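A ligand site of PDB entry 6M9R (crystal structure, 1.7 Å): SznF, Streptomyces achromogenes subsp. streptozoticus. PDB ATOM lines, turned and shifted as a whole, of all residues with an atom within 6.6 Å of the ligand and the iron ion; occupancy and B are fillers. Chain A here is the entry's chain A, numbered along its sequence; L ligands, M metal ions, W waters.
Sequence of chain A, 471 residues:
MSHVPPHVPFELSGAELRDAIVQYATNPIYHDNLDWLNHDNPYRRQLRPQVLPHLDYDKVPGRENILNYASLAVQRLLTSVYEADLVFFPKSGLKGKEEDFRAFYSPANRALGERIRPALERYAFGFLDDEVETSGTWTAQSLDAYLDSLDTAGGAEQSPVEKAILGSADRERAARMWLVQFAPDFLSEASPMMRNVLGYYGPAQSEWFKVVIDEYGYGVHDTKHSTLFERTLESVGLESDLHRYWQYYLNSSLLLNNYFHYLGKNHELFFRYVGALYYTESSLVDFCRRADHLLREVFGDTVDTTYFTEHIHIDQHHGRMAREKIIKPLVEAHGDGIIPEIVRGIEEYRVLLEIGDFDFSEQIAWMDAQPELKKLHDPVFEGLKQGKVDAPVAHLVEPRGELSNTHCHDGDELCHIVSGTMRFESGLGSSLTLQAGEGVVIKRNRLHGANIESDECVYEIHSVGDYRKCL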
ATOM      1  N   ASP A  32      22.493  37.851   5.052  1.00  0.00           N
ATOM      2  CA  ASP A  32      21.308  37.008   4.909  1.00  0.00           C
ATOM      3  C   ASP A  32      20.222  37.699   4.079  1.00  0.00           C
ATOM      4  O   ASP A  32      19.933  38.889   4.241  1.00  0.00           O
ATOM      5  CB  ASP A  32      20.718  36.658   6.295  1.00  0.00           C
ATOM      6  CG  ASP A  32      21.515  35.587   7.055  1.00  0.00           C
ATOM      7  OD1 ASP A  32      22.507  35.031   6.535  1.00  0.00           O
ATOM      8  OD2 ASP A  32      21.136  35.329   8.227  1.00  0.00           O
ATOM      9  N   ARG A  48      26.233  33.692   5.167  1.00  0.00           N
ATOM     10  CA  ARG A  48      25.963  33.613   6.606  1.00  0.00           C
ATOM     11  C   ARG A  48      27.178  34.040   7.431  1.00  0.00           C
ATOM     12  O   ARG A  48      27.685  33.281   8.266  1.00  0.00           O
ATOM     13  CB  ARG A  48      25.428  32.225   7.008  1.00  0.00           C
ATOM     14  CG  ARG A  48      24.126  31.885   6.292  1.00  0.00           C
ATOM     15  CD  ARG A  48      23.531  30.565   6.756  1.00  0.00           C
ATOM     16  NE  ARG A  48      22.857  30.642   8.052  1.00  0.00           N
ATOM     17  CZ  ARG A  48      23.172  29.958   9.156  1.00  0.00           C
ATOM     18  NH1 ARG A  48      24.222  29.129   9.180  1.00  0.00           N
ATOM     19  NH2 ARG A  48      22.444  30.108  10.254  1.00  0.00           N
ATOM     20  N   GLN A  50      27.682  35.849   9.935  1.00  0.00           N
ATOM     21  CA  GLN A  50      27.561  35.812  11.388  1.00  0.00           C
ATOM     22  C   GLN A  50      28.069  34.519  12.045  1.00  0.00           C
ATOM     23  O   GLN A  50      28.453  34.526  13.216  1.00  0.00           O
ATOM     24  CB  GLN A  50      26.108  36.140  11.830  1.00  0.00           C
ATOM     25  CG  GLN A  50      25.053  35.099  11.458  1.00  0.00           C
ATOM     26  CD  GLN A  50      24.571  35.178  10.012  1.00  0.00           C
ATOM     27  OE1 GLN A  50      25.107  35.924   9.193  1.00  0.00           O
ATOM     28  NE2 GLN A  50      23.544  34.407   9.702  1.00  0.00           N
ATOM     29  N   VAL A  51      28.090  33.415  11.296  1.00  0.00           N
ATOM     30  CA  VAL A  51      28.551  32.123  11.823  1.00  0.00           C
ATOM     31  C   VAL A  51      30.073  31.939  11.619  1.00  0.00           C
ATOM     32  O   VAL A  51      30.725  31.191  12.346  1.00  0.00           O
ATOM     33  CB  VAL A  51      27.784  30.940  11.196  1.00  0.00           C
ATOM     34  CG1 VAL A  51      28.124  29.619  11.884  1.00  0.00           C
ATOM     35  CG2 VAL A  51      26.283  31.179  11.285  1.00  0.00           C
ATOM     36  N   LEU A 396      15.493  30.153  21.580  1.00  0.00           N
ATOM     37  CA  LEU A 396      15.445  31.203  20.580  1.00  0.00           C
ATOM     38  C   LEU A 396      14.099  31.924  20.580  1.00  0.00           C
ATOM     39  O   LEU A 396      13.073  31.307  20.815  1.00  0.00           O
ATOM     40  CB  LEU A 396      15.701  30.617  19.192  1.00  0.00           C
ATOM     41  CG  LEU A 396      17.073  29.948  18.997  1.00  0.00           C
ATOM     42  CD1 LEU A 396      17.185  29.395  17.590  1.00  0.00           C
ATOM     43  CD2 LEU A 396      18.229  30.880  19.319  1.00  0.00           C
ATOM     44  N   GLU A 398      12.340  34.870  17.996  1.00  0.00           N
ATOM     45  CA  GLU A 398      12.548  35.537  16.713  1.00  0.00           C
ATOM     46  C   GLU A 398      11.260  36.184  16.210  1.00  0.00           C
ATOM     47  O   GLU A 398      10.180  35.605  16.316  1.00  0.00           O
ATOM     48  CB  GLU A 398      13.098  34.544  15.672  1.00  0.00           C
ATOM     49  CG  GLU A 398      14.471  33.985  16.050  1.00  0.00           C
ATOM     50  CD  GLU A 398      15.060  33.019  15.042  1.00  0.00           C
ATOM     51  OE1 GLU A 398      14.318  32.366  14.296  1.00  0.00           O
ATOM     52  OE2 GLU A 398      16.310  32.923  15.007  1.00  0.00           O
ATOM     53  N   GLU A 402      12.032  36.975  10.352  1.00  0.00           N
ATOM     54  CA  GLU A 402      13.429  36.632  10.545  1.00  0.00           C
ATOM     55  C   GLU A 402      13.667  35.297   9.851  1.00  0.00           C
ATOM     56  O   GLU A 402      13.282  34.226  10.346  1.00  0.00           O
ATOM     57  CB  GLU A 402      13.837  36.543  12.020  1.00  0.00           C
ATOM     58  CG  GLU A 402      15.314  36.165  12.188  1.00  0.00           C
ATOM     59  CD  GLU A 402      16.053  36.962  13.251  1.00  0.00           C
ATOM     60  OE1 GLU A 402      15.421  37.696  14.044  1.00  0.00           O
ATOM     61  OE2 GLU A 402      17.291  36.892  13.266  1.00  0.00           O
ATOM     62  N   LEU A 403      14.245  35.373   8.655  1.00  0.00           N
ATOM     63  CA  LEU A 403      14.419  34.199   7.824  1.00  0.00           C
ATOM     64  C   LEU A 403      15.807  33.627   8.080  1.00  0.00           C
ATOM     65  O   LEU A 403      16.820  34.294   7.797  1.00  0.00           O
ATOM     66  CB  LEU A 403      14.214  34.561   6.353  1.00  0.00           C
ATOM     67  CG  LEU A 403      13.964  33.390   5.405  1.00  0.00           C
ATOM     68  CD1 LEU A 403      13.290  33.876   4.134  1.00  0.00           C
ATOM     69  CD2 LEU A 403      15.259  32.654   5.061  1.00  0.00           C
ATOM     70  N   SER A 404      15.839  32.418   8.641  1.00  0.00           N
ATOM     71  CA  SER A 404      17.070  31.695   8.891  1.00  0.00           C
ATOM     72  C   SER A 404      17.489  31.115   7.546  1.00  0.00           C
ATOM     73  O   SER A 404      16.868  30.196   7.044  1.00  0.00           O
ATOM     74  CB  SER A 404      16.868  30.560   9.893  1.00  0.00           C
ATOM     75  OG  SER A 404      16.352  31.058  11.120  1.00  0.00           O
ATOM     76  N   ASN A 405      18.518  31.714   6.972  1.00  0.00           N
ATOM     77  CA  ASN A 405      19.011  31.286   5.661  1.00  0.00           C
ATOM     78  C   ASN A 405      19.508  29.848   5.761  1.00  0.00           C
ATOM     79  O   ASN A 405      19.951  29.405   6.828  1.00  0.00           O
ATOM     80  CB  ASN A 405      20.103  32.228   5.133  1.00  0.00           C
ATOM     81  CG  ASN A 405      19.565  33.544   4.556  1.00  0.00           C
ATOM     82  OD1 ASN A 405      20.121  34.073   3.596  1.00  0.00           O
ATOM     83  ND2 ASN A 405      18.502  34.082   5.139  1.00  0.00           N
ATOM     84  N   HIS A 407      21.107  26.167   5.903  1.00  0.00           N
ATOM     85  CA  HIS A 407      22.337  25.685   6.512  1.00  0.00           C
ATOM     86  C   HIS A 407      22.126  24.215   6.891  1.00  0.00           C
ATOM     87  O   HIS A 407      21.126  23.610   6.513  1.00  0.00           O
ATOM     88  CB  HIS A 407      22.650  26.533   7.741  1.00  0.00           C
ATOM     89  CG  HIS A 407      21.545  26.538   8.749  1.00  0.00           C
ATOM     90  ND1 HIS A 407      20.469  27.395   8.646  1.00  0.00           N
ATOM     91  CD2 HIS A 407      21.298  25.739   9.814  1.00  0.00           C
ATOM     92  CE1 HIS A 407      19.613  27.136   9.609  1.00  0.00           C
ATOM     93  NE2 HIS A 407      20.096  26.142  10.335  1.00  0.00           N
ATOM     94  N   CYS A 408      23.066  23.648   7.626  1.00  0.00           N
ATOM     95  CA  CYS A 408      22.886  22.329   8.208  1.00  0.00           C
ATOM     96  C   CYS A 408      23.597  22.281   9.545  1.00  0.00           C
ATOM     97  O   CYS A 408      24.316  23.218   9.898  1.00  0.00           O
ATOM     98  CB  CYS A 408      23.396  21.242   7.258  1.00  0.00           C
ATOM     99  SG  CYS A 408      25.198  21.207   7.086  1.00  0.00           S
ATOM    100  N   HIS A 409      23.345  21.203  10.288  1.00  0.00           N
ATOM    101  CA  HIS A 409      24.005  20.938  11.564  1.00  0.00           C
ATOM    102  C   HIS A 409      24.771  19.626  11.464  1.00  0.00           C
ATOM    103  O   HIS A 409      24.474  18.790  10.625  1.00  0.00           O
ATOM    104  CB  HIS A 409      22.980  20.930  12.672  1.00  0.00           C
ATOM    105  CG  HIS A 409      22.171  22.191  12.704  1.00  0.00           C
ATOM    106  ND1 HIS A 409      22.727  23.420  12.996  1.00  0.00           N
ATOM    107  CD2 HIS A 409      20.865  22.415  12.434  1.00  0.00           C
ATOM    108  CE1 HIS A 409      21.790  24.347  12.911  1.00  0.00           C
ATOM    109  NE2 HIS A 409      20.656  23.773  12.567  1.00  0.00           N
ATOM    110  N   GLU A 413      19.185  17.327  15.269  1.00  0.00           N
ATOM    111  CA  GLU A 413      18.631  18.363  16.152  1.00  0.00           C
ATOM    112  C   GLU A 413      17.126  18.230  16.218  1.00  0.00           C
ATOM    113  O   GLU A 413      16.494  17.872  15.243  1.00  0.00           O
ATOM    114  CB  GLU A 413      19.014  19.767  15.661  1.00  0.00           C
ATOM    115  CG  GLU A 413      20.508  19.961  15.421  1.00  0.00           C
ATOM    116  CD  GLU A 413      21.339  20.183  16.679  1.00  0.00           C
ATOM    117  OE1 GLU A 413      22.390  19.498  16.819  1.00  0.00           O
ATOM    118  OE2 GLU A 413      20.992  20.989  17.564  1.00  0.00           O
ATOM    119  N   CYS A 415      13.825  20.480  16.712  1.00  0.00           N
ATOM    120  CA  CYS A 415      13.215  21.801  16.757  1.00  0.00           C
ATOM    121  C   CYS A 415      11.852  21.679  17.417  1.00  0.00           C
ATOM    122  O   CYS A 415      11.010  20.907  16.947  1.00  0.00           O
ATOM    123  CB  CYS A 415      13.077  22.365  15.348  1.00  0.00           C
ATOM    124  SG  CYS A 415      12.276  23.992  15.269  1.00  0.00           S
ATOM    125  N   MET A 422       6.040  28.824  12.541  1.00  0.00           N
ATOM    126  CA  MET A 422       7.265  28.767  11.745  1.00  0.00           C
ATOM    127  C   MET A 422       7.002  28.043  10.422  1.00  0.00           C
ATOM    128  O   MET A 422       6.353  27.005  10.393  1.00  0.00           O
ATOM    129  CB  MET A 422       8.362  28.016  12.526  1.00  0.00           C
ATOM    130  CG  MET A 422       9.675  27.821  11.784  1.00  0.00           C
ATOM    131  SD  MET A 422      10.841  26.782  12.700  1.00  0.00           S
ATOM    132  CE  MET A 422      11.362  27.922  13.980  1.00  0.00           C
ATOM    133  N   PHE A 424       9.045  25.878   8.169  1.00  0.00           N
ATOM    134  CA  PHE A 424      10.284  25.120   8.195  1.00  0.00           C
ATOM    135  C   PHE A 424      10.577  24.577   6.801  1.00  0.00           C
ATOM    136  O   PHE A 424       9.798  23.808   6.253  1.00  0.00           O
ATOM    137  CB  PHE A 424      10.218  23.988   9.217  1.00  0.00           C
ATOM    138  CG  PHE A 424      11.487  23.210   9.318  1.00  0.00           C
ATOM    139  CD1 PHE A 424      12.562  23.696  10.035  1.00  0.00           C
ATOM    140  CD2 PHE A 424      11.634  22.011   8.616  1.00  0.00           C
ATOM    141  CE1 PHE A 424      13.766  22.998  10.095  1.00  0.00           C
ATOM    142  CE2 PHE A 424      12.835  21.305   8.680  1.00  0.00           C
ATOM    143  CZ  PHE A 424      13.895  21.801   9.410  1.00  0.00           C
ATOM    144  N   ILE A 442      15.396  17.274  12.851  1.00  0.00           N
ATOM    145  CA  ILE A 442      16.275  17.788  11.789  1.00  0.00           C
ATOM    146  C   ILE A 442      17.496  16.868  11.645  1.00  0.00           C
ATOM    147  O   ILE A 442      18.346  16.784  12.538  1.00  0.00           O
ATOM    148  CB  ILE A 442      16.776  19.221  12.072  1.00  0.00           C
ATOM    149  CG1 ILE A 442      15.610  20.161  12.346  1.00  0.00           C
ATOM    150  CG2 ILE A 442      17.555  19.772  10.875  1.00  0.00           C
ATOM    151  CD1 ILE A 442      16.028  21.547  12.795  1.00  0.00           C
ATOM    152  N   HIS A 448      18.495  22.961   5.335  1.00  0.00           N
ATOM    153  CA  HIS A 448      17.208  23.442   5.823  1.00  0.00           C
ATOM    154  C   HIS A 448      17.312  24.893   6.264  1.00  0.00           C
ATOM    155  O   HIS A 448      18.393  25.405   6.514  1.00  0.00           O
ATOM    156  CB  HIS A 448      16.754  22.583   7.000  1.00  0.00           C
ATOM    157  CG  HIS A 448      17.575  22.763   8.231  1.00  0.00           C
ATOM    158  ND1 HIS A 448      18.793  22.165   8.396  1.00  0.00           N
ATOM    159  CD2 HIS A 448      17.388  23.544   9.316  1.00  0.00           C
ATOM    160  CE1 HIS A 448      19.315  22.536   9.559  1.00  0.00           C
ATOM    161  NE2 HIS A 448      18.488  23.392  10.118  1.00  0.00           N
ATOM    162  N   GLY A 449      16.154  25.545   6.360  1.00  0.00           N
ATOM    163  CA  GLY A 449      16.068  26.891   6.923  1.00  0.00           C
ATOM    164  C   GLY A 449      14.689  27.105   7.514  1.00  0.00           C
ATOM    165  O   GLY A 449      13.907  26.153   7.643  1.00  0.00           O
ATOM    166  N   ALA A 450      14.385  28.348   7.885  1.00  0.00           N
ATOM    167  CA  ALA A 450      13.067  28.655   8.446  1.00  0.00           C
ATOM    168  C   ALA A 450      12.720  30.127   8.316  1.00  0.00           C
ATOM    169  O   ALA A 450      13.588  30.974   8.163  1.00  0.00           O
ATOM    170  CB  ALA A 450      13.022  28.237   9.908  1.00  0.00           C
ATOM    171  N   TYR A 459      10.995  29.251  20.297  1.00  0.00           N
ATOM    172  CA  TYR A 459      11.292  27.852  20.028  1.00  0.00           C
ATOM    173  C   TYR A 459      12.626  27.404  20.601  1.00  0.00           C
ATOM    174  O   TYR A 459      13.418  28.220  21.061  1.00  0.00           O
ATOM    175  CB  TYR A 459      11.203  27.570  18.512  1.00  0.00           C
ATOM    176  CG  TYR A 459      12.255  28.172  17.607  1.00  0.00           C
ATOM    177  CD1 TYR A 459      12.141  29.471  17.118  1.00  0.00           C
ATOM    178  CD2 TYR A 459      13.338  27.412  17.174  1.00  0.00           C
ATOM    179  CE1 TYR A 459      13.090  30.010  16.258  1.00  0.00           C
ATOM    180  CE2 TYR A 459      14.292  27.929  16.320  1.00  0.00           C
ATOM    181  CZ  TYR A 459      14.166  29.236  15.865  1.00  0.00           C
ATOM    182  OH  TYR A 459      15.145  29.716  14.994  1.00  0.00           O
ATOM    183  N   ILE A 461      15.988  24.543  20.103  1.00  0.00           N
ATOM    184  CA  ILE A 461      16.749  23.571  19.318  1.00  0.00           C
ATOM    185  C   ILE A 461      17.519  22.688  20.299  1.00  0.00           C
ATOM    186  O   ILE A 461      18.399  23.168  21.027  1.00  0.00           O
ATOM    187  CB  ILE A 461      17.717  24.253  18.334  1.00  0.00           C
ATOM    188  CG1 ILE A 461      16.955  25.157  17.355  1.00  0.00           C
ATOM    189  CG2 ILE A 461      18.547  23.224  17.569  1.00  0.00           C
ATOM    190  CD1 ILE A 461      16.087  24.417  16.359  1.00  0.00           C
HETATM  191  N1  LIG L   1      17.997  32.514  12.972  1.00  0.00           N
HETATM  192  C1  LIG L   1      19.252  31.909  13.449  1.00  0.00           C
HETATM  193  C2  LIG L   1      19.121  30.639  14.298  1.00  0.00           C
HETATM  194  C3  LIG L   1      20.174  31.602  12.254  1.00  0.00           C
HETATM  195  O1  LIG L   1      19.736  31.846  11.101  1.00  0.00           O
HETATM  196  C4  LIG L   1      18.451  29.524  13.481  1.00  0.00           C
HETATM  197  C5  LIG L   1      18.424  28.315  14.407  1.00  0.00           C
HETATM  198  N2  LIG L   1      18.333  27.077  13.564  1.00  0.00           N
HETATM  199  C6  LIG L   1      17.194  26.558  13.035  1.00  0.00           C
HETATM  200  N3  LIG L   1      15.993  27.131  13.229  1.00  0.00           N
HETATM  201  N4  LIG L   1      17.274  25.449  12.313  1.00  0.00           N
HETATM  202  O2  LIG L   1      21.274  31.115  12.540  1.00  0.00           O
HETATM  203  C7  LIG L   1      14.716  26.618  12.700  1.00  0.00           C
HETATM  204  O3  LIG L   1      19.599  26.396  13.298  1.00  0.00           O
HETATM  205 FE    FE M   1      19.110  24.831  11.725  1.00  0.00          FE
HETATM  206  O   HOH W   1      21.904  27.979  12.787  1.00  0.00           O
HETATM  207  O   HOH W   2      20.698  32.626   8.618  1.00  0.00           O
HETATM  208  O   HOH W   3      20.715  25.725  15.578  1.00  0.00           O
HETATM  209  O   HOH W   4      22.481  33.317  11.884  1.00  0.00           O
HETATM  210  O   HOH W   5      18.703  34.934  11.948  1.00  0.00           O
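The iron ion is bound by a nitrogen (N4) of the ligand (2.0 Å), a ring nitrogen (NE2) of His 409 (2.1 Å), a ring nitrogen (NE2) of His 407 (2.2 Å), a ring nitrogen (NE2) of His 448 (2.2 Å) and an oxygen (O3) of the ligand (2.3 Å). The iron ion has five donor atoms within binding distance.
The side-chain carboxylate (OE2) of Glu 398 is in salt-bridge range of a nitrogen (N1) of the ligand (2.7 Å). The guanidinium group (NH2) of Arg 48 is in salt-bridge range of an oxygen (O2) of the ligand (2.8 Å). OG of Ser 404 sits at hydrogen-bond distance from N1 of the ligand (2.9 Å). N3 of the ligand is in hydrogen-bond range of OH of Tyr 459 (3.2 Å).
Merely in contact with the ligand: Leu 396 (3.6 Å), Met 422 (3.8 Å) and Ala 450 (3.6 Å). The nearest printed residue that does not touch the ligand is Ile 461 (4.1 Å).
ND1 of His 407 is in hydrogen-bond range of O of Asn 405, at 2.8 Å. OH of Tyr 459 sits at hydrogen-bond distance from OE1 of Glu 398 (2.9 Å). O of Asn 405 is in hydrogen-bond range of NE of Arg 48 (3.4 Å). The backbone carbonyl oxygen of Ala 450 is in hydrogen-bond range of the backbone NH of Ser 404, 2.7 Å away. The backbone carbonyl oxygen (O) of Tyr 459 lies within hydrogen-bond range of the backbone NH (N) of Leu 396 (2.9 Å).
Water W4 lies within hydrogen-bond range of an oxygen (O2) of the ligand (2.6 Å) and the side-chain amide nitrogen (NE2) of Gln 50 (2.7 Å). Water W5 lies within hydrogen-bond range of a nitrogen (N1) of the ligand (2.7 Å) and the side-chain carboxylate (OE2) of Glu 402 (2.8 Å). Water W2 lies within hydrogen-bond range of the side-chain carboxylate of Asp 32 (2.8 Å), an oxygen (O1) of the ligand (2.8 Å), the backbone NH of Asn 405 (2.9 Å) and the guanidinium group of Arg 48 (3.0 Å). Water W1 bridges O2 of the ligand (3.2 Å) and NH2 of Arg 48 (3.4 Å).
Of the 23 residues printed, 3 come within 4 Å of the iron ion. The nearest printed residue that does not touch the iron ion is Ile 442 (4.6 Å).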
